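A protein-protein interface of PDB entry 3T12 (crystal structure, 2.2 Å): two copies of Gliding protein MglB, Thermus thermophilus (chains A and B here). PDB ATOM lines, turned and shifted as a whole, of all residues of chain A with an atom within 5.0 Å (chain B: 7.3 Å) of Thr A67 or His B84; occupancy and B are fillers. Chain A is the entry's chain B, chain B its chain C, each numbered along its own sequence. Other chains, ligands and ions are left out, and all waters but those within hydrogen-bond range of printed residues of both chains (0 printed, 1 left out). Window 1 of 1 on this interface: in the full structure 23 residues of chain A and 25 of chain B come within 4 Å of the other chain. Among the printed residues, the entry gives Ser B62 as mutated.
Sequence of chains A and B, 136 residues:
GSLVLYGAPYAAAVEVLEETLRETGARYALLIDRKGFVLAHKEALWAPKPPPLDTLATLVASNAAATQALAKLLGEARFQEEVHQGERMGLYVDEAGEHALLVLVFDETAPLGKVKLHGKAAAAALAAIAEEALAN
The side-chain amide oxygen (OD1) of Asn B63 lies close to the side-chain amide oxygen (OD1) of Asn A63.
The backbone carbonyl oxygen (O) of Asn A63 lies close to the side-chain hydroxyl (OG1) of Thr A67, at 3.3 Å.
OG of Ser B62 lies within hydrogen-bond range of O of Leu B59 (3.0 Å).
The backbone carbonyl oxygen of Ala A64 lies within hydrogen-bond range of the side-chain hydroxyl of Thr A67, at 3.2 Å.
The backbone NH (N) of His B84 sits at hydrogen-bond distance from the backbone carbonyl oxygen (O) of Leu B91 (2.9 Å).
The side-chain amide nitrogen (ND2) of Asn B63 lies close to a ring nitrogen (NE2) of His B84 (3.3 Å).
O of Asn B63 sits close to OG1 of Thr B67, 3.4 Å away.
Among the printed residues, merely in contact across the chains: Asn A63 with Thr B67 (3.2 Å), Phe A79 with Gln B85 (3.5 Å), Phe A79 with Gly B86 (3.5 Å), Leu A70 with Leu B59 (3.6 Å), Thr A67 with Asn B63 (3.6 Å), Phe A79 with His B84 (3.6 Å), Ala A66 with Ser B62 (3.8 Å), Leu A70 with Val B60 (3.9 Å), Ala A69 with Leu B59 (3.9 Å), Leu A70 with Leu B91 (3.9 Å) and Thr A67 with His B84 (3.9 Å).
Of the printed residues of chain B, Ala A66 touches Ser B62.
Thr A67 touches just these residues of chain B: Asn B63 and His B84.
Printed residues of chain B within 4 Å of Leu A70: Leu B59 (3.6 Å), Val B60 (3.9 Å) and Leu B91 (3.9 Å).
Glu A82 touches none of the printed residues of chain B.
Of the printed residues of chain A, Leu B59 touches Ala A69 and Leu A70.
Ala B64 touches none of the printed residues of chain A.
Of the printed residues of chain A, Thr B67 touches Asn A63.
Of chain A, only Thr A67 (3.9 Å) and Phe A79 (3.6 Å) come within 4 Å of His B84.
The nearest residue of chain B that does not touch Thr A67 is Leu B59 (5.8 Å).
The nearest residue of chain A that does not touch His B84 is Leu A70 (4.6 Å).
The nearest printed residue of chain A that does not touch Gly B86 is Ala A71 (6.7 Å).
Hydrophobic or aromatic side chains of chain A that line the printed part of chain B: Ala A66, Ala A69, Leu A70 and Phe A79.
Hydrophobic or aromatic side chains of chain B within 4 Å of the printed part of chain A: Leu B59, Val B60, His B84 and Leu B91.
Among the printed residues, 12 pairs touch across the chains.
Among the printed residues, no Asp or Glu carboxylate lies within 4 Å of a Lys or Arg side-chain nitrogen of the other chain.
Asn A63 touches its own counterpart, Asn B63.
Asn A63 touches Thr B67, and with the chains exchanged Thr A67 touches Asn B63.
Positions printed for both chains: 63, 64, 67 and 82.
Of the 12 pairs that touch across the chains among the printed residues, 3 have their exchanged pair printed and touching as well.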
ATOM      1  N   ASN A  63      37.092  -5.068  11.939  1.00  0.00           N
ATOM      2  CA  ASN A  63      35.673  -4.813  11.976  1.00  0.00           C
ATOM      3  C   ASN A  63      34.814  -5.867  11.273  1.00  0.00           C
ATOM      4  O   ASN A  63      33.840  -6.337  11.871  1.00  0.00           O
ATOM      5  CB  ASN A  63      35.332  -3.492  11.366  1.00  0.00           C
ATOM      6  CG  ASN A  63      34.045  -2.938  11.924  1.00  0.00           C
ATOM      7  OD1 ASN A  63      33.781  -2.996  13.146  1.00  0.00           O
ATOM      8  ND2 ASN A  63      33.182  -2.474  11.033  1.00  0.00           N
ATOM      9  N   ALA A  64      35.165  -6.180  10.044  1.00  0.00           N
ATOM     10  CA  ALA A  64      34.475  -7.183   9.262  1.00  0.00           C
ATOM     11  C   ALA A  64      34.517  -8.561   9.928  1.00  0.00           C
ATOM     12  O   ALA A  64      33.556  -9.278   9.835  1.00  0.00           O
ATOM     13  CB  ALA A  64      35.096  -7.329   7.868  1.00  0.00           C
ATOM     14  N   ALA A  65      35.643  -8.948  10.538  1.00  0.00           N
ATOM     15  CA  ALA A  65      35.745 -10.292  11.109  1.00  0.00           C
ATOM     16  C   ALA A  65      34.797 -10.367  12.332  1.00  0.00           C
ATOM     17  O   ALA A  65      34.224 -11.444  12.595  1.00  0.00           O
ATOM     18  CB  ALA A  65      37.162 -10.557  11.579  1.00  0.00           C
ATOM     19  N   ALA A  66      34.734  -9.254  13.080  1.00  0.00           N
ATOM     20  CA  ALA A  66      33.902  -9.098  14.257  1.00  0.00           C
ATOM     21  C   ALA A  66      32.391  -9.057  13.869  1.00  0.00           C
ATOM     22  O   ALA A  66      31.576  -9.749  14.488  1.00  0.00           O
ATOM     23  CB  ALA A  66      34.244  -7.860  14.950  1.00  0.00           C
ATOM     24  N   THR A  67      32.027  -8.227  12.875  1.00  0.00           N
ATOM     25  CA  THR A  67      30.650  -8.158  12.374  1.00  0.00           C
ATOM     26  C   THR A  67      30.231  -9.437  11.712  1.00  0.00           C
ATOM     27  O   THR A  67      29.081  -9.818  11.799  1.00  0.00           O
ATOM     28  CB  THR A  67      30.402  -6.960  11.411  1.00  0.00           C
ATOM     29  OG1 THR A  67      31.139  -7.194  10.243  1.00  0.00           O
ATOM     30  CG2 THR A  67      30.846  -5.651  11.993  1.00  0.00           C
ATOM     31  N   GLN A  68      31.138 -10.139  11.060  1.00  0.00           N
ATOM     32  CA  GLN A  68      30.822 -11.449  10.493  1.00  0.00           C
ATOM     33  C   GLN A  68      30.575 -12.479  11.599  1.00  0.00           C
ATOM     34  O   GLN A  68      29.712 -13.398  11.456  1.00  0.00           O
ATOM     35  CB  GLN A  68      31.924 -11.917   9.541  1.00  0.00           C
ATOM     36  CG  GLN A  68      31.809 -13.365   9.069  1.00  0.00           C
ATOM     37  CD  GLN A  68      32.636 -13.642   7.827  1.00  0.00           C
ATOM     38  OE1 GLN A  68      33.704 -14.219   7.932  1.00  0.00           O
ATOM     39  NE2 GLN A  68      32.153 -13.199   6.637  1.00  0.00           N
ATOM     40  N   ALA A  69      31.328 -12.351  12.710  1.00  0.00           N
ATOM     41  CA  ALA A  69      31.122 -13.314  13.812  1.00  0.00           C
ATOM     42  C   ALA A  69      29.760 -12.982  14.500  1.00  0.00           C
ATOM     43  O   ALA A  69      29.071 -13.883  14.965  1.00  0.00           O
ATOM     44  CB  ALA A  69      32.283 -13.320  14.805  1.00  0.00           C
ATOM     45  N   LEU A  70      29.401 -11.695  14.568  1.00  0.00           N
ATOM     46  CA  LEU A  70      28.112 -11.323  15.112  1.00  0.00           C
ATOM     47  C   LEU A  70      26.953 -11.915  14.280  1.00  0.00           C
ATOM     48  O   LEU A  70      25.946 -12.346  14.831  1.00  0.00           O
ATOM     49  CB  LEU A  70      27.957  -9.833  15.144  1.00  0.00           C
ATOM     50  CG  LEU A  70      28.582  -9.193  16.356  1.00  0.00           C
ATOM     51  CD1 LEU A  70      28.622  -7.704  16.097  1.00  0.00           C
ATOM     52  CD2 LEU A  70      27.781  -9.537  17.680  1.00  0.00           C
ATOM     53  N   ALA A  71      27.088 -11.863  12.954  1.00  0.00           N
ATOM     54  CA  ALA A  71      26.055 -12.357  12.079  1.00  0.00           C
ATOM     55  C   ALA A  71      25.850 -13.855  12.355  1.00  0.00           C
ATOM     56  O   ALA A  71      24.732 -14.281  12.604  1.00  0.00           O
ATOM     57  CB  ALA A  71      26.415 -12.111  10.564  1.00  0.00           C
ATOM     58  N   PHE A  79      25.453  -9.564   7.436  1.00  0.00           N
ATOM     59  CA  PHE A  79      24.645  -8.350   7.452  1.00  0.00           C
ATOM     60  C   PHE A  79      24.758  -7.589   6.096  1.00  0.00           C
ATOM     61  O   PHE A  79      25.307  -8.088   5.181  1.00  0.00           O
ATOM     62  CB  PHE A  79      25.089  -7.463   8.590  1.00  0.00           C
ATOM     63  CG  PHE A  79      24.963  -8.096   9.972  1.00  0.00           C
ATOM     64  CD1 PHE A  79      23.758  -8.708  10.387  1.00  0.00           C
ATOM     65  CD2 PHE A  79      25.998  -8.018  10.866  1.00  0.00           C
ATOM     66  CE1 PHE A  79      23.631  -9.238  11.653  1.00  0.00           C
ATOM     67  CE2 PHE A  79      25.885  -8.570  12.138  1.00  0.00           C
ATOM     68  CZ  PHE A  79      24.685  -9.162  12.543  1.00  0.00           C
ATOM     69  N   GLU A  82      27.860  -1.491   4.707  1.00  0.00           N
ATOM     70  CA  GLU A  82      27.872  -0.454   5.758  1.00  0.00           C
ATOM     71  C   GLU A  82      28.147   0.925   5.201  1.00  0.00           C
ATOM     72  O   GLU A  82      28.920   1.103   4.269  1.00  0.00           O
ATOM     73  CB  GLU A  82      28.975  -0.776   6.764  1.00  0.00           C
ATOM     74  CG  GLU A  82      28.841  -2.142   7.400  1.00  0.00           C
ATOM     75  CD  GLU A  82      30.081  -2.483   8.258  1.00  0.00           C
ATOM     76  OE1 GLU A  82      30.017  -3.436   9.073  1.00  0.00           O
ATOM     77  OE2 GLU A  82      31.123  -1.774   8.102  1.00  0.00           O
ATOM     78  N   LEU B  59      32.055  -9.173  21.040  1.00  0.00           N
ATOM     79  CA  LEU B  59      31.998  -8.903  19.621  1.00  0.00           C
ATOM     80  C   LEU B  59      31.477  -7.515  19.332  1.00  0.00           C
ATOM     81  O   LEU B  59      32.057  -6.780  18.467  1.00  0.00           O
ATOM     82  CB  LEU B  59      31.113  -9.951  18.873  1.00  0.00           C
ATOM     83  CG  LEU B  59      31.753 -11.349  18.872  1.00  0.00           C
ATOM     84  CD1 LEU B  59      30.736 -12.333  18.228  1.00  0.00           C
ATOM     85  CD2 LEU B  59      33.151 -11.351  18.169  1.00  0.00           C
ATOM     86  N   VAL B  60      30.389  -7.133  20.012  1.00  0.00           N
ATOM     87  CA  VAL B  60      29.832  -5.801  19.864  1.00  0.00           C
ATOM     88  C   VAL B  60      30.822  -4.720  20.355  1.00  0.00           C
ATOM     89  O   VAL B  60      30.987  -3.666  19.718  1.00  0.00           O
ATOM     90  CB  VAL B  60      28.498  -5.575  20.592  1.00  0.00           C
ATOM     91  CG1 VAL B  60      28.091  -4.042  20.511  1.00  0.00           C
ATOM     92  CG2 VAL B  60      27.350  -6.437  19.947  1.00  0.00           C
ATOM     93  N   SER B  62      34.086  -4.831  20.369  1.00  0.00           N
ATOM     94  CA  SER B  62      35.214  -4.716  19.489  1.00  0.00           C
ATOM     95  C   SER B  62      34.842  -4.138  18.058  1.00  0.00           C
ATOM     96  O   SER B  62      35.668  -3.538  17.391  1.00  0.00           O
ATOM     97  CB  SER B  62      35.863  -6.060  19.317  1.00  0.00           C
ATOM     98  OG  SER B  62      35.015  -6.847  18.511  1.00  0.00           O
ATOM     99  N   ASN B  63      33.608  -4.325  17.626  1.00  0.00           N
ATOM    100  CA  ASN B  63      33.005  -3.681  16.499  1.00  0.00           C
ATOM    101  C   ASN B  63      32.967  -2.229  16.704  1.00  0.00           C
ATOM    102  O   ASN B  63      33.478  -1.480  15.841  1.00  0.00           O
ATOM    103  CB  ASN B  63      31.582  -4.254  16.343  1.00  0.00           C
ATOM    104  CG  ASN B  63      30.700  -3.474  15.347  1.00  0.00           C
ATOM    105  OD1 ASN B  63      31.149  -2.941  14.311  1.00  0.00           O
ATOM    106  ND2 ASN B  63      29.435  -3.479  15.642  1.00  0.00           N
ATOM    107  N   ALA B  64      32.407  -1.794  17.837  1.00  0.00           N
ATOM    108  CA  ALA B  64      32.405  -0.399  18.234  1.00  0.00           C
ATOM    109  C   ALA B  64      33.811   0.183  18.418  1.00  0.00           C
ATOM    110  O   ALA B  64      34.007   1.344  18.141  1.00  0.00           O
ATOM    111  CB  ALA B  64      31.684  -0.173  19.551  1.00  0.00           C
ATOM    112  N   THR B  67      35.151   0.687  14.791  1.00  0.00           N
ATOM    113  CA  THR B  67      34.483   1.722  14.032  1.00  0.00           C
ATOM    114  C   THR B  67      34.735   3.103  14.572  1.00  0.00           C
ATOM    115  O   THR B  67      34.841   4.081  13.800  1.00  0.00           O
ATOM    116  CB  THR B  67      32.942   1.466  13.847  1.00  0.00           C
ATOM    117  OG1 THR B  67      32.293   1.635  15.079  1.00  0.00           O
ATOM    118  CG2 THR B  67      32.671   0.041  13.334  1.00  0.00           C
ATOM    119  N   GLU B  82      24.598   2.289  15.042  1.00  0.00           N
ATOM    120  CA  GLU B  82      24.684   1.296  14.027  1.00  0.00           C
ATOM    121  C   GLU B  82      23.475   0.310  14.080  1.00  0.00           C
ATOM    122  O   GLU B  82      23.040  -0.106  15.182  1.00  0.00           O
ATOM    123  CB  GLU B  82      26.025   0.564  14.210  1.00  0.00           C
ATOM    124  CG  GLU B  82      26.253  -0.629  13.307  1.00  0.00           C
ATOM    125  CD  GLU B  82      26.603  -0.233  11.891  1.00  0.00           C
ATOM    126  OE1 GLU B  82      25.709   0.274  11.167  1.00  0.00           O
ATOM    127  OE2 GLU B  82      27.760  -0.466  11.487  1.00  0.00           O
ATOM    128  N   VAL B  83      22.953  -0.059  12.891  1.00  0.00           N
ATOM    129  CA  VAL B  83      21.971  -1.093  12.792  1.00  0.00           C
ATOM    130  C   VAL B  83      22.533  -2.131  11.910  1.00  0.00           C
ATOM    131  O   VAL B  83      22.737  -1.880  10.705  1.00  0.00           O
ATOM    132  CB  VAL B  83      20.653  -0.598  12.174  1.00  0.00           C
ATOM    133  CG1 VAL B  83      19.673  -1.773  11.941  1.00  0.00           C
ATOM    134  CG2 VAL B  83      20.003   0.448  13.036  1.00  0.00           C
ATOM    135  N   HIS B  84      22.785  -3.305  12.464  1.00  0.00           N
ATOM    136  CA  HIS B  84      23.260  -4.400  11.677  1.00  0.00           C
ATOM    137  C   HIS B  84      22.011  -5.193  11.301  1.00  0.00           C
ATOM    138  O   HIS B  84      21.258  -5.577  12.183  1.00  0.00           O
ATOM    139  CB  HIS B  84      24.229  -5.301  12.450  1.00  0.00           C
ATOM    140  CG  HIS B  84      25.524  -4.658  12.835  1.00  0.00           C
ATOM    141  ND1 HIS B  84      25.865  -4.376  14.162  1.00  0.00           N
ATOM    142  CD2 HIS B  84      26.588  -4.290  12.083  1.00  0.00           C
ATOM    143  CE1 HIS B  84      27.068  -3.833  14.194  1.00  0.00           C
ATOM    144  NE2 HIS B  84      27.539  -3.807  12.952  1.00  0.00           N
ATOM    145  N   GLN B  85      21.804  -5.482  10.014  1.00  0.00           N
ATOM    146  CA  GLN B  85      20.579  -6.108   9.567  1.00  0.00           C
ATOM    147  C   GLN B  85      20.779  -7.362   8.794  1.00  0.00           C
ATOM    148  O   GLN B  85      21.307  -7.341   7.683  1.00  0.00           O
ATOM    149  CB  GLN B  85      19.788  -5.094   8.760  1.00  0.00           C
ATOM    150  CG  GLN B  85      18.464  -5.674   8.263  1.00  0.00           C
ATOM    151  CD  GLN B  85      17.414  -5.833   9.388  1.00  0.00           C
ATOM    152  OE1 GLN B  85      16.865  -4.826   9.845  1.00  0.00           O
ATOM    153  NE2 GLN B  85      17.092  -7.106   9.770  1.00  0.00           N
ATOM    154  N   GLY B  86      20.379  -8.496   9.363  1.00  0.00           N
ATOM    155  CA  GLY B  86      20.432  -9.735   8.616  1.00  0.00           C
ATOM    156  C   GLY B  86      19.077  -9.945   7.894  1.00  0.00           C
ATOM    157  O   GLY B  86      18.197  -9.055   7.887  1.00  0.00           O
ATOM    158  N   MET B  89      17.354 -11.603  11.809  1.00  0.00           N
ATOM    159  CA  MET B  89      17.929 -11.008  13.032  1.00  0.00           C
ATOM    160  C   MET B  89      18.639  -9.675  12.791  1.00  0.00           C
ATOM    161  O   MET B  89      19.296  -9.519  11.759  1.00  0.00           O
ATOM    162  CB  MET B  89      18.904 -11.961  13.662  1.00  0.00           C
ATOM    163  CG  MET B  89      18.395 -13.358  13.969  1.00  0.00           C
ATOM    164  SD  MET B  89      16.910 -13.250  15.007  1.00  0.00           S
ATOM    165  CE  MET B  89      17.475 -12.605  16.612  1.00  0.00           C
ATOM    166  N   GLY B  90      18.559  -8.742  13.741  1.00  0.00           N
ATOM    167  CA  GLY B  90      19.396  -7.539  13.707  1.00  0.00           C
ATOM    168  C   GLY B  90      19.899  -7.065  15.057  1.00  0.00           C
ATOM    169  O   GLY B  90      19.504  -7.647  16.096  1.00  0.00           O
ATOM    170  N   LEU B  91      20.688  -5.979  15.061  1.00  0.00           N
ATOM    171  CA  LEU B  91      21.276  -5.394  16.275  1.00  0.00           C
ATOM    172  C   LEU B  91      21.269  -3.923  16.137  1.00  0.00           C
ATOM    173  O   LEU B  91      21.650  -3.390  15.088  1.00  0.00           O
ATOM    174  CB  LEU B  91      22.772  -5.685  16.388  1.00  0.00           C
ATOM    175  CG  LEU B  91      23.272  -7.012  16.787  1.00  0.00           C
ATOM    176  CD1 LEU B  91      22.606  -7.962  15.934  1.00  0.00           C
ATOM    177  CD2 LEU B  91      24.806  -7.093  16.484  1.00  0.00           C
ATOM    178  N   TYR B  92      20.874  -3.253  17.189  1.00  0.00           N
ATOM    179  CA  TYR B  92      20.906  -1.832  17.267  1.00  0.00           C
ATOM    180  C   TYR B  92      21.934  -1.562  18.357  1.00  0.00           C
ATOM    181  O   TYR B  92      21.791  -2.136  19.472  1.00  0.00           O
ATOM    182  CB  TYR B  92      19.552  -1.252  17.666  1.00  0.00           C
ATOM    183  CG  TYR B  92      19.596   0.262  17.940  1.00  0.00           C
ATOM    184  CD1 TYR B  92      19.338   1.183  16.944  1.00  0.00           C
ATOM    185  CD2 TYR B  92      19.879   0.739  19.197  1.00  0.00           C
ATOM    186  CE1 TYR B  92      19.381   2.583  17.197  1.00  0.00           C
ATOM    187  CE2 TYR B  92      19.972   2.103  19.473  1.00  0.00           C
ATOM    188  CZ  TYR B  92      19.694   3.031  18.446  1.00  0.00           C
ATOM    189  OH  TYR B  92      19.758   4.399  18.720  1.00  0.00           O
ATOM    190  N   VAL B  93      22.943  -0.701  18.052  1.00  0.00           N
ATOM    191  CA  VAL B  93      24.069  -0.448  18.934  1.00  0.00           C
ATOM    192  C   VAL B  93      24.233   1.039  19.001  1.00  0.00           C
ATOM    193  O   VAL B  93      24.418   1.704  17.987  1.00  0.00           O
ATOM    194  CB  VAL B  93      25.381  -1.130  18.450  1.00  0.00           C
ATOM    195  CG1 VAL B  93      26.524  -0.912  19.420  1.00  0.00           C
ATOM    196  CG2 VAL B  93      25.192  -2.653  18.376  1.00  0.00           C
ATOM    197  N   LEU B 104      20.533  -3.660  21.430  1.00  0.00           N
ATOM    198  CA  LEU B 104      19.236  -4.308  21.259  1.00  0.00           C
ATOM    199  C   LEU B 104      19.332  -5.376  20.221  1.00  0.00           C
ATOM    200  O   LEU B 104      19.857  -5.145  19.096  1.00  0.00           O
ATOM    201  CB  LEU B 104      18.168  -3.301  20.843  1.00  0.00           C
ATOM    202  CG  LEU B 104      17.950  -2.226  21.890  1.00  0.00           C
ATOM    203  CD1 LEU B 104      16.909  -1.189  21.419  1.00  0.00           C
ATOM    204  CD2 LEU B 104      17.447  -2.877  23.199  1.00  0.00           C
ATOM    205  N   PHE B 106      16.964  -7.853  17.990  1.00  0.00           N
ATOM    206  CA  PHE B 106      15.574  -7.871  17.559  1.00  0.00           C
ATOM    207  C   PHE B 106      15.437  -8.819  16.409  1.00  0.00           C
ATOM    208  O   PHE B 106      16.454  -9.227  15.802  1.00  0.00           O
ATOM    209  CB  PHE B 106      15.059  -6.487  17.204  1.00  0.00           C
ATOM    210  CG  PHE B 106      15.800  -5.796  16.063  1.00  0.00           C
ATOM    211  CD1 PHE B 106      15.372  -5.954  14.719  1.00  0.00           C
ATOM    212  CD2 PHE B 106      16.912  -4.962  16.328  1.00  0.00           C
ATOM    213  CE1 PHE B 106      16.047  -5.281  13.618  1.00  0.00           C
ATOM    214  CE2 PHE B 106      17.619  -4.316  15.246  1.00  0.00           C
ATOM    215  CZ  PHE B 106      17.181  -4.488  13.904  1.00  0.00           C
